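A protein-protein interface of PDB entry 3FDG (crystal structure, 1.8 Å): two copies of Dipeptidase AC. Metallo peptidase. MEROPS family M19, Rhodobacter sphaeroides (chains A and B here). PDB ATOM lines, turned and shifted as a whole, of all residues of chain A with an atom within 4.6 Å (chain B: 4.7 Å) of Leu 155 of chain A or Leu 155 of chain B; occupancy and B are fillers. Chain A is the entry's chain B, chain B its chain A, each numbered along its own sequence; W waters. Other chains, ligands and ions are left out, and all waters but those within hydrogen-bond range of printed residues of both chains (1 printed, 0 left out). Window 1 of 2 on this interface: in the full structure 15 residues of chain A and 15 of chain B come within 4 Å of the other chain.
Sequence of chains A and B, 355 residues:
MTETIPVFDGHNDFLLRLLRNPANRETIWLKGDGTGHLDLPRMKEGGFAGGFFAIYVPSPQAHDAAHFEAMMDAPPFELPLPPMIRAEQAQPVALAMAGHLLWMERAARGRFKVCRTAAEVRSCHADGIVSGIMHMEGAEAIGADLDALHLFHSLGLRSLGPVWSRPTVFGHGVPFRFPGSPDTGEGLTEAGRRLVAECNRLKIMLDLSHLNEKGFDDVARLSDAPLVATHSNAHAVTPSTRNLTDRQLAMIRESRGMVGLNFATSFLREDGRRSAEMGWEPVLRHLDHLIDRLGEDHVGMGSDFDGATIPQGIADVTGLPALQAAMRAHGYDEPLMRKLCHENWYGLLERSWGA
Water W1 lies within hydrogen-bond range of O of Ser 154 of chain A (2.5 Å) and O of Ser 154 of chain B (2.6 Å).
Leu 151 of chain A touches Leu 155 of chain B, but with the chains exchanged Leu 155 of chain A does not touch Leu 151 of chain B (4.2 Å).
Ser 154 of chain B touches its own counterpart, Ser 154 of chain A.
Leu 155 of chain A touches Ser 154 of chain B, but with the chains exchanged Ser 154 of chain A does not touch Leu 155 of chain B (4.1 Å).
Leu 155 of chain A touches its own counterpart, Leu 155 of chain B.
Positions printed for both chains: 116, 134, 151, 152, 153, 154, 155, 156 and 157.
Of chain B, only Ser 154 and Leu 155 come within 4 Å of Leu 155 of chain A.
Printed residues of chain A within 4 Å of Leu 155 of chain B: Leu 151 and Leu 155.
Printed residues of chain B within 4 Å of Leu 151 of chain A: Leu 95, Leu 102 and Leu 155.
Printed residues of chain A within 4 Å of Leu 95 of chain B: Leu 151 (2.9 Å).
Of the printed residues of chain A, Leu 102 of chain B touches Leu 151 (3.8 Å) and Ser 154 (3.7 Å).
C of Ala 98 of chain A touches CD2 of Leu 151 of chain B, at 3.9 Å.
CD1 of Leu 151 of chain A touches O of Leu 95 of chain B (2.9 Å).
CD2 of Leu 151 of chain A touches CD1 of Leu 102 of chain B (3.8 Å).
Leu 155 of chain B touches Leu 151 of chain A (CD2 to O, 2.9 Å).
Leu 102 of chain B touches Ser 154 of chain A (CD1 to OG, 3.7 Å).
Ser 154 of chain A touches Ser 154 of chain B.
Ser 154 of chain B touches Leu 155 of chain A (CB to CB, 3.8 Å).
Leu 155 of chain A touches Leu 155 of chain B (CD2 to CD2, 3.7 Å).
The backbone carbonyl oxygen (O) of Leu 155 of chain B is in hydrogen-bond range of the guanidinium group (NH2) of Arg 116 of chain B (3.0 Å).
O of Leu 155 of chain A sits at hydrogen-bond distance from NH2 of Arg 116 of chain A (2.8 Å).
Printed residues of chain A that touch a printed residue of chain B: Ala 98, Leu 151, Ser 154 and Leu 155.
Hydrophobic or aromatic side chains of chain A within 4 Å of the printed part of chain B: Ala 98, Leu 151 and Leu 155.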
ATOM      1  N   ALA A  98       0.505  19.073   1.393  1.00  0.00           N
ATOM      2  CA  ALA A  98       1.765  18.599   0.881  1.00  0.00           C
ATOM      3  C   ALA A  98       1.572  17.897  -0.470  1.00  0.00           C
ATOM      4  O   ALA A  98       2.362  18.099  -1.423  1.00  0.00           O
ATOM      5  CB  ALA A  98       2.484  17.665   1.932  1.00  0.00           C
ATOM      6  N   ARG A 116      14.851  21.694  -2.215  1.00  0.00           N
ATOM      7  CA  ARG A 116      15.234  21.181  -0.887  1.00  0.00           C
ATOM      8  C   ARG A 116      16.568  21.706  -0.435  1.00  0.00           C
ATOM      9  O   ARG A 116      16.987  21.446   0.721  1.00  0.00           O
ATOM     10  CB  ARG A 116      15.270  19.618  -0.929  1.00  0.00           C
ATOM     11  CG  ARG A 116      13.855  19.003  -1.154  1.00  0.00           C
ATOM     12  CD  ARG A 116      13.958  17.431  -1.367  1.00  0.00           C
ATOM     13  NE  ARG A 116      12.620  16.821  -1.345  1.00  0.00           N
ATOM     14  CZ  ARG A 116      11.699  16.948  -2.311  1.00  0.00           C
ATOM     15  NH1 ARG A 116      11.941  17.634  -3.432  1.00  0.00           N
ATOM     16  NH2 ARG A 116      10.500  16.360  -2.162  1.00  0.00           N
ATOM     17  N   MET A 134       8.805  23.866   0.746  1.00  0.00           N
ATOM     18  CA  MET A 134       7.736  23.312   1.568  1.00  0.00           C
ATOM     19  C   MET A 134       7.904  23.789   3.007  1.00  0.00           C
ATOM     20  O   MET A 134       8.915  23.455   3.705  1.00  0.00           O
ATOM     21  CB  MET A 134       7.671  21.757   1.441  1.00  0.00           C
ATOM     22  CG  MET A 134       6.548  21.081   2.276  1.00  0.00           C
ATOM     23  SD  MET A 134       6.631  19.192   2.265  1.00  0.00           S
ATOM     24  CE  MET A 134       6.407  18.851   0.479  1.00  0.00           C
ATOM     25  N   LEU A 151       9.527  12.363   9.132  1.00  0.00           N
ATOM     26  CA  LEU A 151       8.755  12.021   7.924  1.00  0.00           C
ATOM     27  C   LEU A 151       8.570  13.192   6.964  1.00  0.00           C
ATOM     28  O   LEU A 151       8.851  13.082   5.737  1.00  0.00           O
ATOM     29  CB  LEU A 151       7.355  11.434   8.310  1.00  0.00           C
ATOM     30  CG  LEU A 151       7.103  10.114   9.056  1.00  0.00           C
ATOM     31  CD1 LEU A 151       5.623   9.780   9.473  1.00  0.00           C
ATOM     32  CD2 LEU A 151       7.813   8.962   8.385  1.00  0.00           C
ATOM     33  N   PHE A 152       8.085  14.311   7.506  1.00  0.00           N
ATOM     34  CA  PHE A 152       7.883  15.507   6.657  1.00  0.00           C
ATOM     35  C   PHE A 152       9.230  15.976   6.061  1.00  0.00           C
ATOM     36  O   PHE A 152       9.322  16.343   4.873  1.00  0.00           O
ATOM     37  CB  PHE A 152       7.128  16.627   7.421  1.00  0.00           C
ATOM     38  CG  PHE A 152       5.615  16.416   7.417  1.00  0.00           C
ATOM     39  CD1 PHE A 152       4.869  16.741   6.272  1.00  0.00           C
ATOM     40  CD2 PHE A 152       4.957  15.860   8.507  1.00  0.00           C
ATOM     41  CE1 PHE A 152       3.456  16.555   6.202  1.00  0.00           C
ATOM     42  CE2 PHE A 152       3.533  15.636   8.466  1.00  0.00           C
ATOM     43  CZ  PHE A 152       2.790  16.004   7.292  1.00  0.00           C
ATOM     44  N   HIS A 153      10.295  15.875   6.839  1.00  0.00           N
ATOM     45  CA  HIS A 153      11.610  16.310   6.278  1.00  0.00           C
ATOM     46  C   HIS A 153      12.000  15.444   5.058  1.00  0.00           C
ATOM     47  O   HIS A 153      12.523  15.933   4.026  1.00  0.00           O
ATOM     48  CB  HIS A 153      12.692  16.238   7.381  1.00  0.00           C
ATOM     49  CG  HIS A 153      14.041  16.628   6.905  1.00  0.00           C
ATOM     50  ND1 HIS A 153      14.906  15.719   6.338  1.00  0.00           N
ATOM     51  CD2 HIS A 153      14.621  17.842   6.770  1.00  0.00           C
ATOM     52  CE1 HIS A 153      15.992  16.351   5.933  1.00  0.00           C
ATOM     53  NE2 HIS A 153      15.835  17.640   6.166  1.00  0.00           N
ATOM     54  N   SER A 154      11.743  14.140   5.172  1.00  0.00           N
ATOM     55  CA  SER A 154      12.055  13.216   4.084  1.00  0.00           C
ATOM     56  C   SER A 154      11.272  13.558   2.876  1.00  0.00           C
ATOM     57  O   SER A 154      11.761  13.380   1.762  1.00  0.00           O
ATOM     58  CB  SER A 154      11.753  11.756   4.479  1.00  0.00           C
ATOM     59  OG  SER A 154      12.615  11.411   5.534  1.00  0.00           O
ATOM     60  N   LEU A 155      10.051  14.037   3.040  1.00  0.00           N
ATOM     61  CA  LEU A 155       9.339  14.379   1.840  1.00  0.00           C
ATOM     62  C   LEU A 155       9.574  15.785   1.298  1.00  0.00           C
ATOM     63  O   LEU A 155       9.068  16.124   0.213  1.00  0.00           O
ATOM     64  CB  LEU A 155       7.864  13.971   1.897  1.00  0.00           C
ATOM     65  CG  LEU A 155       6.978  14.514   2.989  1.00  0.00           C
ATOM     66  CD1 LEU A 155       6.552  15.787   2.463  1.00  0.00           C
ATOM     67  CD2 LEU A 155       5.759  13.627   3.185  1.00  0.00           C
ATOM     68  N   GLY A 156      10.352  16.595   2.020  1.00  0.00           N
ATOM     69  CA  GLY A 156      10.821  17.881   1.497  1.00  0.00           C
ATOM     70  C   GLY A 156      10.589  19.104   2.381  1.00  0.00           C
ATOM     71  O   GLY A 156      10.960  20.200   2.010  1.00  0.00           O
ATOM     72  N   LEU A 157      10.063  18.914   3.594  1.00  0.00           N
ATOM     73  CA  LEU A 157       9.792  20.055   4.493  1.00  0.00           C
ATOM     74  C   LEU A 157      11.151  20.676   4.902  1.00  0.00           C
ATOM     75  O   LEU A 157      12.058  19.950   5.352  1.00  0.00           O
ATOM     76  CB  LEU A 157       9.007  19.568   5.737  1.00  0.00           C
ATOM     77  CG  LEU A 157       8.733  20.697   6.790  1.00  0.00           C
ATOM     78  CD1 LEU A 157       7.578  21.488   6.220  1.00  0.00           C
ATOM     79  CD2 LEU A 157       8.369  20.113   8.145  1.00  0.00           C
ATOM     80  N   LEU B  95       1.087   6.918   8.807  1.00  0.00           N
ATOM     81  CA  LEU B  95       2.211   7.820   9.197  1.00  0.00           C
ATOM     82  C   LEU B  95       2.883   7.422  10.482  1.00  0.00           C
ATOM     83  O   LEU B  95       4.106   7.597  10.645  1.00  0.00           O
ATOM     84  CB  LEU B  95       1.783   9.262   9.359  1.00  0.00           C
ATOM     85  CG  LEU B  95       1.494   9.956   8.025  1.00  0.00           C
ATOM     86  CD1 LEU B  95       0.868  11.318   8.380  1.00  0.00           C
ATOM     87  CD2 LEU B  95       2.766  10.161   7.128  1.00  0.00           C
ATOM     88  N   LEU B 102      11.369   4.800  10.434  1.00  0.00           N
ATOM     89  CA  LEU B 102      12.496   5.761  10.342  1.00  0.00           C
ATOM     90  C   LEU B 102      13.172   5.824  11.705  1.00  0.00           C
ATOM     91  O   LEU B 102      14.410   5.803  11.798  1.00  0.00           O
ATOM     92  CB  LEU B 102      12.066   7.164   9.816  1.00  0.00           C
ATOM     93  CG  LEU B 102      11.504   7.349   8.390  1.00  0.00           C
ATOM     94  CD1 LEU B 102      11.571   8.870   8.001  1.00  0.00           C
ATOM     95  CD2 LEU B 102      12.156   6.501   7.341  1.00  0.00           C
ATOM     96  N   ARG B 116      16.250   2.301  -0.584  1.00  0.00           N
ATOM     97  CA  ARG B 116      15.308   2.848  -1.582  1.00  0.00           C
ATOM     98  C   ARG B 116      15.747   2.390  -2.935  1.00  0.00           C
ATOM     99  O   ARG B 116      15.057   2.688  -3.937  1.00  0.00           O
ATOM    100  CB  ARG B 116      15.317   4.400  -1.512  1.00  0.00           C
ATOM    101  CG  ARG B 116      14.738   4.966  -0.181  1.00  0.00           C
ATOM    102  CD  ARG B 116      14.851   6.590  -0.037  1.00  0.00           C
ATOM    103  NE  ARG B 116      14.155   7.096   1.184  1.00  0.00           N
ATOM    104  CZ  ARG B 116      14.488   6.821   2.466  1.00  0.00           C
ATOM    105  NH1 ARG B 116      15.538   6.073   2.794  1.00  0.00           N
ATOM    106  NH2 ARG B 116      13.748   7.315   3.472  1.00  0.00           N
ATOM    107  N   MET B 134      10.498  -0.116   2.879  1.00  0.00           N
ATOM    108  CA  MET B 134       9.206   0.402   3.273  1.00  0.00           C
ATOM    109  C   MET B 134       8.125  -0.100   2.325  1.00  0.00           C
ATOM    110  O   MET B 134       8.139   0.204   1.116  1.00  0.00           O
ATOM    111  CB  MET B 134       9.239   1.951   3.254  1.00  0.00           C
ATOM    112  CG  MET B 134       7.905   2.589   3.765  1.00  0.00           C
ATOM    113  SD  MET B 134       7.925   4.439   3.842  1.00  0.00           S
ATOM    114  CE  MET B 134       9.182   4.674   5.166  1.00  0.00           C
ATOM    115  N   LEU B 151       3.611  11.268  -2.267  1.00  0.00           N
ATOM    116  CA  LEU B 151       4.176  11.615  -0.934  1.00  0.00           C
ATOM    117  C   LEU B 151       4.864  10.452  -0.248  1.00  0.00           C
ATOM    118  O   LEU B 151       6.015  10.566   0.257  1.00  0.00           O
ATOM    119  CB  LEU B 151       3.050  12.120   0.008  1.00  0.00           C
ATOM    120  CG  LEU B 151       2.428  13.452  -0.380  1.00  0.00           C
ATOM    121  CD1 LEU B 151       1.309  13.755   0.618  1.00  0.00           C
ATOM    122  CD2 LEU B 151       3.569  14.556  -0.309  1.00  0.00           C
ATOM    123  N   PHE B 152       4.172   9.309  -0.218  1.00  0.00           N
ATOM    124  CA  PHE B 152       4.789   8.099   0.357  1.00  0.00           C
ATOM    125  C   PHE B 152       6.028   7.712  -0.400  1.00  0.00           C
ATOM    126  O   PHE B 152       7.039   7.302   0.202  1.00  0.00           O
ATOM    127  CB  PHE B 152       3.754   6.940   0.475  1.00  0.00           C
ATOM    128  CG  PHE B 152       2.898   7.068   1.726  1.00  0.00           C
ATOM    129  CD1 PHE B 152       3.429   6.695   2.990  1.00  0.00           C
ATOM    130  CD2 PHE B 152       1.615   7.576   1.658  1.00  0.00           C
ATOM    131  CE1 PHE B 152       2.664   6.840   4.188  1.00  0.00           C
ATOM    132  CE2 PHE B 152       0.811   7.732   2.823  1.00  0.00           C
ATOM    133  CZ  PHE B 152       1.331   7.365   4.093  1.00  0.00           C
ATOM    134  N   HIS B 153       5.986   7.857  -1.724  1.00  0.00           N
ATOM    135  CA  HIS B 153       7.188   7.518  -2.505  1.00  0.00           C
ATOM    136  C   HIS B 153       8.396   8.400  -2.092  1.00  0.00           C
ATOM    137  O   HIS B 153       9.533   7.947  -2.026  1.00  0.00           O
ATOM    138  CB  HIS B 153       6.905   7.734  -4.005  1.00  0.00           C
ATOM    139  CG  HIS B 153       8.042   7.331  -4.859  1.00  0.00           C
ATOM    140  ND1 HIS B 153       8.955   8.250  -5.336  1.00  0.00           N
ATOM    141  CD2 HIS B 153       8.502   6.104  -5.219  1.00  0.00           C
ATOM    142  CE1 HIS B 153       9.904   7.603  -5.996  1.00  0.00           C
ATOM    143  NE2 HIS B 153       9.651   6.305  -5.941  1.00  0.00           N
ATOM    144  N   SER B 154       8.144   9.678  -1.847  1.00  0.00           N
ATOM    145  CA  SER B 154       9.192  10.560  -1.389  1.00  0.00           C
ATOM    146  C   SER B 154       9.720  10.147  -0.069  1.00  0.00           C
ATOM    147  O   SER B 154      10.908  10.356   0.166  1.00  0.00           O
ATOM    148  CB  SER B 154       8.661  11.975  -1.203  1.00  0.00           C
ATOM    149  OG  SER B 154       8.448  12.454  -2.479  1.00  0.00           O
ATOM    150  N   LEU B 155       8.872   9.581   0.790  1.00  0.00           N
ATOM    151  CA  LEU B 155       9.304   9.127   2.153  1.00  0.00           C
ATOM    152  C   LEU B 155      10.162   7.889   2.093  1.00  0.00           C
ATOM    153  O   LEU B 155      10.771   7.481   3.129  1.00  0.00           O
ATOM    154  CB  LEU B 155       8.098   8.749   3.052  1.00  0.00           C
ATOM    155  CG  LEU B 155       7.068   9.782   3.423  1.00  0.00           C
ATOM    156  CD1 LEU B 155       5.899   9.110   4.151  1.00  0.00           C
ATOM    157  CD2 LEU B 155       7.791  10.781   4.334  1.00  0.00           C
ATOM    158  N   GLY B 156      10.145   7.203   0.946  1.00  0.00           N
ATOM    159  CA  GLY B 156      10.856   5.921   0.806  1.00  0.00           C
ATOM    160  C   GLY B 156      10.034   4.669   0.483  1.00  0.00           C
ATOM    161  O   GLY B 156      10.587   3.587   0.319  1.00  0.00           O
ATOM    162  N   LEU B 157       8.730   4.836   0.222  1.00  0.00           N
ATOM    163  CA  LEU B 157       7.874   3.655  -0.011  1.00  0.00           C
ATOM    164  C   LEU B 157       8.307   3.066  -1.369  1.00  0.00           C
ATOM    165  O   LEU B 157       8.391   3.798  -2.375  1.00  0.00           O
ATOM    166  CB  LEU B 157       6.380   4.113  -0.092  1.00  0.00           C
ATOM    167  CG  LEU B 157       5.430   2.939  -0.405  1.00  0.00           C
ATOM    168  CD1 LEU B 157       5.273   2.117   0.831  1.00  0.00           C
ATOM    169  CD2 LEU B 157       4.056   3.497  -0.889  1.00  0.00           C
HETATM  170  O   HOH W   1      12.384  12.427  -0.495  1.00  0.00           O
